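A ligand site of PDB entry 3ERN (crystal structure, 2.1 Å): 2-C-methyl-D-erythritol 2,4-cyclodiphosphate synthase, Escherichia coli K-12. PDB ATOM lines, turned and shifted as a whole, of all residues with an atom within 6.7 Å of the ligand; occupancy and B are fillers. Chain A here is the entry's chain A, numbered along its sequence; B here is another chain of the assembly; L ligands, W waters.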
ATOM      1  N   ILE A 104      -7.908   7.373 -27.380  1.00  0.00           N
ATOM      2  CA  ILE A 104      -6.877   6.390 -27.723  1.00  0.00           C
ATOM      3  C   ILE A 104      -7.214   5.100 -27.018  1.00  0.00           C
ATOM      4  O   ILE A 104      -7.457   5.090 -25.818  1.00  0.00           O
ATOM      5  CB  ILE A 104      -5.476   6.880 -27.307  1.00  0.00           C
ATOM      6  CG1 ILE A 104      -5.197   8.255 -27.944  1.00  0.00           C
ATOM      7  CG2 ILE A 104      -4.392   5.851 -27.671  1.00  0.00           C
ATOM      8  CD1 ILE A 104      -4.195   9.092 -27.161  1.00  0.00           C
ATOM      9  N   ILE A 105      -7.236   4.009 -27.767  1.00  0.00           N
ATOM     10  CA  ILE A 105      -7.560   2.715 -27.193  1.00  0.00           C
ATOM     11  C   ILE A 105      -6.294   1.846 -27.235  1.00  0.00           C
ATOM     12  O   ILE A 105      -5.876   1.424 -28.299  1.00  0.00           O
ATOM     13  CB  ILE A 105      -8.770   2.083 -27.923  1.00  0.00           C
ATOM     14  CG1 ILE A 105      -9.913   3.119 -27.998  1.00  0.00           C
ATOM     15  CG2 ILE A 105      -9.239   0.846 -27.213  1.00  0.00           C
ATOM     16  CD1 ILE A 105     -11.132   2.685 -28.774  1.00  0.00           C
ATOM     17  N   ALA A 106      -5.671   1.642 -26.074  1.00  0.00           N
ATOM     18  CA  ALA A 106      -4.404   0.897 -25.960  1.00  0.00           C
ATOM     19  C   ALA A 106      -4.218   0.320 -24.573  1.00  0.00           C
ATOM     20  O   ALA A 106      -4.539   0.970 -23.584  1.00  0.00           O
ATOM     21  CB  ALA A 106      -3.229   1.783 -26.275  1.00  0.00           C
ATOM     22  N   GLN A 107      -3.675  -0.894 -24.478  1.00  0.00           N
ATOM     23  CA  GLN A 107      -3.354  -1.482 -23.183  1.00  0.00           C
ATOM     24  C   GLN A 107      -2.054  -0.882 -22.626  1.00  0.00           C
ATOM     25  O   GLN A 107      -1.893  -0.696 -21.429  1.00  0.00           O
ATOM     26  CB  GLN A 107      -3.209  -3.011 -23.311  1.00  0.00           C
ATOM     27  CG  GLN A 107      -3.239  -3.744 -21.976  1.00  0.00           C
ATOM     28  CD  GLN A 107      -4.572  -3.629 -21.284  1.00  0.00           C
ATOM     29  OE1 GLN A 107      -5.618  -3.807 -21.883  1.00  0.00           O
ATOM     30  NE2 GLN A 107      -4.553  -3.314 -19.991  1.00  0.00           N
ATOM     31  N   ALA A 108      -1.131  -0.579 -23.534  1.00  0.00           N
ATOM     32  CA  ALA A 108       0.195  -0.091 -23.203  1.00  0.00           C
ATOM     33  C   ALA A 108       0.621   0.532 -24.503  1.00  0.00           C
ATOM     34  O   ALA A 108       0.103   0.163 -25.533  1.00  0.00           O
ATOM     35  CB  ALA A 108       1.124  -1.263 -22.840  1.00  0.00           C
ATOM     36  N   PRO A 109       1.569   1.494 -24.475  1.00  0.00           N
ATOM     37  CA  PRO A 109       2.198   2.085 -23.306  1.00  0.00           C
ATOM     38  C   PRO A 109       1.261   3.053 -22.603  1.00  0.00           C
ATOM     39  O   PRO A 109       0.131   3.274 -23.086  1.00  0.00           O
ATOM     40  CB  PRO A 109       3.417   2.817 -23.891  1.00  0.00           C
ATOM     41  CG  PRO A 109       3.060   3.110 -25.291  1.00  0.00           C
ATOM     42  CD  PRO A 109       2.079   2.049 -25.731  1.00  0.00           C
ATOM     43  N   LYS A 110       1.706   3.592 -21.478  1.00  0.00           N
ATOM     44  CA  LYS A 110       0.994   4.620 -20.730  1.00  0.00           C
ATOM     45  C   LYS A 110       0.951   5.931 -21.528  1.00  0.00           C
ATOM     46  O   LYS A 110       1.987   6.458 -21.934  1.00  0.00           O
ATOM     47  CB  LYS A 110       1.638   4.851 -19.372  1.00  0.00           C
ATOM     48  CG  LYS A 110       1.382   3.728 -18.372  1.00  0.00           C
ATOM     49  CD  LYS A 110       1.910   4.101 -16.989  1.00  0.00           C
ATOM     50  CE  LYS A 110       2.036   2.850 -16.103  1.00  0.00           C
ATOM     51  NZ  LYS A 110       2.143   3.216 -14.650  1.00  0.00           N
ATOM     52  N   MET A 111      -0.256   6.435 -21.739  1.00  0.00           N
ATOM     53  CA  MET A 111      -0.478   7.632 -22.562  1.00  0.00           C
ATOM     54  C   MET A 111      -0.599   8.904 -21.733  1.00  0.00           C
ATOM     55  O   MET A 111      -0.114   9.951 -22.146  1.00  0.00           O
ATOM     56  CB  MET A 111      -1.737   7.466 -23.416  1.00  0.00           C
ATOM     57  CG  MET A 111      -1.716   6.275 -24.361  1.00  0.00           C
ATOM     58  SD  MET A 111      -0.481   6.459 -25.631  1.00  0.00           S
ATOM     59  CE  MET A 111      -0.790   4.972 -26.586  1.00  0.00           C
ATOM     60  N   LEU A 112      -1.266   8.814 -20.586  1.00  0.00           N
ATOM     61  CA  LEU A 112      -1.634   9.979 -19.767  1.00  0.00           C
ATOM     62  C   LEU A 112      -0.521  11.012 -19.518  1.00  0.00           C
ATOM     63  O   LEU A 112      -0.765  12.213 -19.676  1.00  0.00           O
ATOM     64  CB  LEU A 112      -2.316   9.545 -18.455  1.00  0.00           C
ATOM     65  CG  LEU A 112      -2.873  10.566 -17.466  1.00  0.00           C
ATOM     66  CD1 LEU A 112      -3.983  11.450 -18.054  1.00  0.00           C
ATOM     67  CD2 LEU A 112      -3.359   9.856 -16.208  1.00  0.00           C
ATOM     68  N   PRO A 113       0.697  10.560 -19.141  1.00  0.00           N
ATOM     69  CA  PRO A 113       1.823  11.486 -18.989  1.00  0.00           C
ATOM     70  C   PRO A 113       2.145  12.302 -20.238  1.00  0.00           C
ATOM     71  O   PRO A 113       2.700  13.393 -20.127  1.00  0.00           O
ATOM     72  CB  PRO A 113       3.007  10.557 -18.684  1.00  0.00           C
ATOM     73  CG  PRO A 113       2.389   9.365 -18.058  1.00  0.00           C
ATOM     74  CD  PRO A 113       1.085   9.178 -18.780  1.00  0.00           C
ATOM     75  N   ILE A 115      -0.231  13.084 -22.678  1.00  0.00           N
ATOM     76  CA  ILE A 115      -1.431  13.746 -23.242  1.00  0.00           C
ATOM     77  C   ILE A 115      -1.403  15.301 -23.290  1.00  0.00           C
ATOM     78  O   ILE A 115      -1.818  15.882 -24.297  1.00  0.00           O
ATOM     79  CB  ILE A 115      -2.767  13.235 -22.612  1.00  0.00           C
ATOM     80  CG1 ILE A 115      -3.089  11.830 -23.134  1.00  0.00           C
ATOM     81  CG2 ILE A 115      -3.921  14.198 -22.919  1.00  0.00           C
ATOM     82  CD1 ILE A 115      -4.376  11.230 -22.570  1.00  0.00           C
ATOM     83  N   LYS A 136      -8.190  11.687 -24.530  1.00  0.00           N
ATOM     84  CA  LYS A 136      -8.228  10.717 -23.437  1.00  0.00           C
ATOM     85  C   LYS A 136      -7.679   9.362 -23.919  1.00  0.00           C
ATOM     86  O   LYS A 136      -7.519   9.137 -25.124  1.00  0.00           O
ATOM     87  CB  LYS A 136      -9.642  10.592 -22.861  1.00  0.00           C
ATOM     88  CG  LYS A 136     -10.662   9.945 -23.791  1.00  0.00           C
ATOM     89  CD  LYS A 136     -12.103  10.136 -23.307  1.00  0.00           C
ATOM     90  CE  LYS A 136     -12.754  11.368 -23.916  1.00  0.00           C
ATOM     91  NZ  LYS A 136     -12.922  11.246 -25.393  1.00  0.00           N
ATOM     92  N   ALA A 137      -7.384   8.478 -22.981  1.00  0.00           N
ATOM     93  CA  ALA A 137      -6.915   7.131 -23.337  1.00  0.00           C
ATOM     94  C   ALA A 137      -7.559   6.101 -22.431  1.00  0.00           C
ATOM     95  O   ALA A 137      -7.774   6.355 -21.243  1.00  0.00           O
ATOM     96  CB  ALA A 137      -5.410   7.074 -23.269  1.00  0.00           C
ATOM     97  N   THR A 138      -7.889   4.941 -22.985  1.00  0.00           N
ATOM     98  CA  THR A 138      -8.523   3.887 -22.196  1.00  0.00           C
ATOM     99  C   THR A 138      -7.910   2.535 -22.554  1.00  0.00           C
ATOM    100  O   THR A 138      -7.389   2.383 -23.647  1.00  0.00           O
ATOM    101  CB  THR A 138     -10.054   3.853 -22.425  1.00  0.00           C
ATOM    102  OG1 THR A 138     -10.675   2.946 -21.503  1.00  0.00           O
ATOM    103  CG2 THR A 138     -10.407   3.428 -23.853  1.00  0.00           C
ATOM    104  N   THR A 139      -7.958   1.589 -21.626  1.00  0.00           N
ATOM    105  CA  THR A 139      -7.589   0.197 -21.921  1.00  0.00           C
ATOM    106  C   THR A 139      -8.871  -0.545 -22.308  1.00  0.00           C
ATOM    107  O   THR A 139      -9.975   0.023 -22.249  1.00  0.00           O
ATOM    108  CB  THR A 139      -6.925  -0.507 -20.704  1.00  0.00           C
ATOM    109  OG1 THR A 139      -7.910  -0.742 -19.676  1.00  0.00           O
ATOM    110  CG2 THR A 139      -5.776   0.318 -20.113  1.00  0.00           C
ATOM    111  N   THR A 140      -8.724  -1.800 -22.733  1.00  0.00           N
ATOM    112  CA  THR A 140      -9.863  -2.696 -22.951  1.00  0.00           C
ATOM    113  C   THR A 140      -9.838  -3.840 -21.944  1.00  0.00           C
ATOM    114  O   THR A 140     -10.324  -4.939 -22.231  1.00  0.00           O
ATOM    115  CB  THR A 140      -9.944  -3.249 -24.399  1.00  0.00           C
ATOM    116  OG1 THR A 140      -8.696  -3.876 -24.755  1.00  0.00           O
ATOM    117  CG2 THR A 140     -10.260  -2.139 -25.387  1.00  0.00           C
ATOM    118  N   GLU A 141      -9.266  -3.570 -20.777  1.00  0.00           N
ATOM    119  CA  GLU A 141      -9.133  -4.532 -19.676  1.00  0.00           C
ATOM    120  C   GLU A 141      -8.561  -5.891 -20.105  1.00  0.00           C
ATOM    121  O   GLU A 141      -9.051  -6.927 -19.684  1.00  0.00           O
ATOM    122  CB  GLU A 141     -10.448  -4.710 -18.936  1.00  0.00           C
ATOM    123  CG  GLU A 141     -11.095  -3.381 -18.557  1.00  0.00           C
ATOM    124  CD  GLU A 141     -11.944  -3.503 -17.324  1.00  0.00           C
ATOM    125  OE1 GLU A 141     -12.553  -4.566 -17.098  1.00  0.00           O
ATOM    126  OE2 GLU A 141     -12.012  -2.505 -16.568  1.00  0.00           O
ATOM    127  N   ASP B  14     -15.807   2.572 -23.174  1.00  0.00           N
ATOM    128  CA  ASP B  14     -15.358   1.812 -22.002  1.00  0.00           C
ATOM    129  C   ASP B  14     -15.507   0.309 -22.209  1.00  0.00           C
ATOM    130  O   ASP B  14     -16.307  -0.140 -23.042  1.00  0.00           O
ATOM    131  CB  ASP B  14     -16.107   2.243 -20.734  1.00  0.00           C
ATOM    132  CG  ASP B  14     -15.489   1.671 -19.456  1.00  0.00           C
ATOM    133  OD1 ASP B  14     -14.245   1.538 -19.372  1.00  0.00           O
ATOM    134  OD2 ASP B  14     -16.242   1.326 -18.513  1.00  0.00           O
ATOM    135  N   VAL B  15     -14.729  -0.461 -21.452  1.00  0.00           N
ATOM    136  CA  VAL B  15     -14.776  -1.921 -21.528  1.00  0.00           C
ATOM    137  C   VAL B  15     -14.713  -2.516 -20.125  1.00  0.00           C
ATOM    138  O   VAL B  15     -13.901  -2.097 -19.307  1.00  0.00           O
ATOM    139  CB  VAL B  15     -13.639  -2.468 -22.406  1.00  0.00           C
ATOM    140  CG1 VAL B  15     -13.481  -4.001 -22.239  1.00  0.00           C
ATOM    141  CG2 VAL B  15     -13.860  -2.113 -23.857  1.00  0.00           C
ATOM    142  N   HIS B  48     -19.696   4.935 -17.327  1.00  0.00           N
ATOM    143  CA  HIS B  48     -18.296   5.298 -17.521  1.00  0.00           C
ATOM    144  C   HIS B  48     -18.045   5.924 -18.881  1.00  0.00           C
ATOM    145  O   HIS B  48     -17.304   6.910 -18.979  1.00  0.00           O
ATOM    146  CB  HIS B  48     -17.393   4.060 -17.373  1.00  0.00           C
ATOM    147  CG  HIS B  48     -15.920   4.356 -17.352  1.00  0.00           C
ATOM    148  ND1 HIS B  48     -15.073   3.832 -16.401  1.00  0.00           N
ATOM    149  CD2 HIS B  48     -15.143   5.102 -18.185  1.00  0.00           C
ATOM    150  CE1 HIS B  48     -13.835   4.242 -16.630  1.00  0.00           C
ATOM    151  NE2 HIS B  48     -13.853   5.015 -17.710  1.00  0.00           N
ATOM    152  N   ASP B  52     -17.089   9.977 -19.586  1.00  0.00           N
ATOM    153  CA  ASP B  52     -15.944  10.349 -20.441  1.00  0.00           C
ATOM    154  C   ASP B  52     -16.359  11.257 -21.611  1.00  0.00           C
ATOM    155  O   ASP B  52     -15.618  12.191 -21.975  1.00  0.00           O
ATOM    156  CB  ASP B  52     -15.277   9.098 -21.011  1.00  0.00           C
ATOM    157  CG  ASP B  52     -14.247   8.478 -20.058  1.00  0.00           C
ATOM    158  OD1 ASP B  52     -14.168   8.858 -18.871  1.00  0.00           O
ATOM    159  OD2 ASP B  52     -13.499   7.598 -20.510  1.00  0.00           O
ATOM    160  N   ASP B  62     -10.942  13.002 -18.739  1.00  0.00           N
ATOM    161  CA  ASP B  62     -11.744  11.779 -18.583  1.00  0.00           C
ATOM    162  C   ASP B  62     -11.946  11.445 -17.107  1.00  0.00           C
ATOM    163  O   ASP B  62     -11.475  12.176 -16.237  1.00  0.00           O
ATOM    164  CB  ASP B  62     -11.102  10.610 -19.347  1.00  0.00           C
ATOM    165  CG  ASP B  62      -9.771  10.151 -18.752  1.00  0.00           C
ATOM    166  OD1 ASP B  62      -9.284  10.743 -17.762  1.00  0.00           O
ATOM    167  OD2 ASP B  62      -9.200   9.173 -19.281  1.00  0.00           O
ATOM    168  N   ILE B  63     -12.655  10.359 -16.823  1.00  0.00           N
ATOM    169  CA  ILE B  63     -12.827   9.881 -15.437  1.00  0.00           C
ATOM    170  C   ILE B  63     -11.476   9.677 -14.743  1.00  0.00           C
ATOM    171  O   ILE B  63     -11.275  10.153 -13.632  1.00  0.00           O
ATOM    172  CB  ILE B  63     -13.695   8.584 -15.367  1.00  0.00           C
ATOM    173  CG1 ILE B  63     -15.170   8.951 -15.210  1.00  0.00           C
ATOM    174  CG2 ILE B  63     -13.262   7.683 -14.207  1.00  0.00           C
ATOM    175  CD1 ILE B  63     -16.109   7.743 -15.226  1.00  0.00           C
ATOM    176  N   GLY B  64     -10.575   8.998 -15.394  1.00  0.00           N
ATOM    177  CA  GLY B  64      -9.273   8.730 -14.845  1.00  0.00           C
ATOM    178  C   GLY B  64      -8.472   9.958 -14.527  1.00  0.00           C
ATOM    179  O   GLY B  64      -7.641   9.903 -13.698  1.00  0.00           O
ATOM    180  N   LYS B  65      -8.736  11.076 -15.170  1.00  0.00           N
ATOM    181  CA  LYS B  65      -8.010  12.274 -14.913  1.00  0.00           C
ATOM    182  C   LYS B  65      -8.508  12.983 -13.688  1.00  0.00           C
ATOM    183  O   LYS B  65      -7.731  13.457 -12.920  1.00  0.00           O
ATOM    184  CB  LYS B  65      -8.053  13.205 -16.116  1.00  0.00           C
ATOM    185  CG  LYS B  65      -7.034  14.303 -16.112  1.00  0.00           C
ATOM    186  CD  LYS B  65      -7.623  15.571 -16.591  1.00  0.00           C
ATOM    187  CE  LYS B  65      -6.606  16.545 -17.106  1.00  0.00           C
ATOM    188  NZ  LYS B  65      -6.122  17.449 -16.077  1.00  0.00           N
ATOM    189  N   ASP B  69      -7.198   6.257  -9.809  1.00  0.00           N
ATOM    190  CA  ASP B  69      -7.248   5.084  -8.923  1.00  0.00           C
ATOM    191  C   ASP B  69      -6.259   5.246  -7.770  1.00  0.00           C
ATOM    192  O   ASP B  69      -6.432   4.640  -6.712  1.00  0.00           O
ATOM    193  CB  ASP B  69      -6.971   3.777  -9.699  1.00  0.00           C
ATOM    194  CG  ASP B  69      -5.581   3.732 -10.315  1.00  0.00           C
ATOM    195  OD1 ASP B  69      -4.720   2.996  -9.780  1.00  0.00           O
ATOM    196  OD2 ASP B  69      -5.351   4.434 -11.333  1.00  0.00           O
HETATM  197  P1  LIG L   1      -8.768   2.250 -17.817  1.00  0.00           P
HETATM  198  O1  LIG L   1      -9.036   1.574 -19.117  1.00  0.00           O
HETATM  199  O2  LIG L   1      -7.820   1.365 -16.854  1.00  0.00           O
HETATM  200  O3  LIG L   1     -10.142   2.512 -16.986  1.00  0.00           O
HETATM  201  O4  LIG L   1      -8.032   3.677 -17.962  1.00  0.00           O
HETATM  202  C1  LIG L   1      -7.953   4.536 -16.807  1.00  0.00           C
HETATM  203  C2  LIG L   1      -6.798   5.545 -16.906  1.00  0.00           C
HETATM  204  O5  LIG L   1      -5.588   4.856 -17.267  1.00  0.00           O
HETATM  205  C3  LIG L   1      -7.003   6.549 -18.036  1.00  0.00           C
HETATM  206  O6  LIG L   1      -7.826   7.606 -17.571  1.00  0.00           O
HETATM  207  C4  LIG L   1      -5.590   7.035 -18.255  1.00  0.00           C
HETATM  208  O7  LIG L   1      -5.405   7.459 -19.603  1.00  0.00           O
HETATM  209  C5  LIG L   1      -4.744   5.777 -18.007  1.00  0.00           C
HETATM  210  N1  LIG L   1      -4.263   5.132 -19.271  1.00  0.00           N
HETATM  211  C6  LIG L   1      -3.012   5.512 -19.798  1.00  0.00           C
HETATM  212  O8  LIG L   1      -2.338   6.353 -19.214  1.00  0.00           O
HETATM  213  N2  LIG L   1      -2.547   4.906 -20.977  1.00  0.00           N
HETATM  214  C7  LIG L   1      -3.332   3.944 -21.612  1.00  0.00           C
HETATM  215  N3  LIG L   1      -2.904   3.374 -22.737  1.00  0.00           N
HETATM  216  C8  LIG L   1      -4.567   3.578 -21.106  1.00  0.00           C
HETATM  217  C9  LIG L   1      -5.028   4.174 -19.935  1.00  0.00           C
HETATM  218  O   HOH W   1      -6.808   9.556 -20.131  1.00  0.00           O
HETATM  219  O   HOH W   2     -10.776   4.538 -18.705  1.00  0.00           O
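N of Thr 139 is in hydrogen-bond range of O1 of the ligand (2.7 Å). The side-chain hydroxyl (OG1) of Thr 139 sits at hydrogen-bond distance from an oxygen (O1) of the ligand, at 2.6 Å. O6 of the ligand sits at hydrogen-bond distance from OD2 of Asp 62 of chain B. N of Met 111 sits at hydrogen-bond distance from N2 of the ligand, at 2.9 Å. N of Leu 112 is in hydrogen-bond range of O8 of the ligand, 3.0 Å away. A nitrogen (N3) of the ligand lies within hydrogen-bond range of the backbone carbonyl oxygen of Ala 106 (3.0 Å). The backbone carbonyl oxygen (O) of Pro 109 sits at hydrogen-bond distance from a nitrogen (N3) of the ligand, at 3.1 Å. An oxygen (O7) of the ligand is in hydrogen-bond range of the backbone carbonyl oxygen of Ala 137 (3.1 Å). An oxygen (O1) of the ligand lies within hydrogen-bond range of the side-chain hydroxyl (OG1) of Thr 138.
Water W1 lies within hydrogen-bond range of the side-chain carboxylate of Asp 62 of chain B (2.6 Å), an oxygen (O7) of the ligand (2.6 Å) and the backbone NH of Ala 137 (3.1 Å). Water W2 lies within hydrogen-bond range of an oxygen (O3) of the ligand (2.7 Å), the side-chain hydroxyl of Thr 138 (3.2 Å) and a ring nitrogen (NE2) of His 48 of chain B (3.3 Å).
The side-chain hydroxyl (OG1) of Thr 139 lies within hydrogen-bond range of the backbone NH (N) of Glu 141, at 3.3 Å. The side-chain carboxylate (OD1) of Asp 62 of chain B lies within hydrogen-bond range of the backbone NH (N) of Gly 64 of chain B (3.2 Å). N of Lys 65 of chain B lies within hydrogen-bond range of OD1 of Asp 62 of chain B. O of Thr 138 is in hydrogen-bond range of N of Ala 106, at 3.1 Å. The backbone NH (N) of Thr 138 sits at hydrogen-bond distance from the backbone carbonyl oxygen (O) of Ile 104 (2.9 Å).
Lys 110 touches the ligand. Gly 64 of chain B touches the ligand (CA to O6, 3.3 Å).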
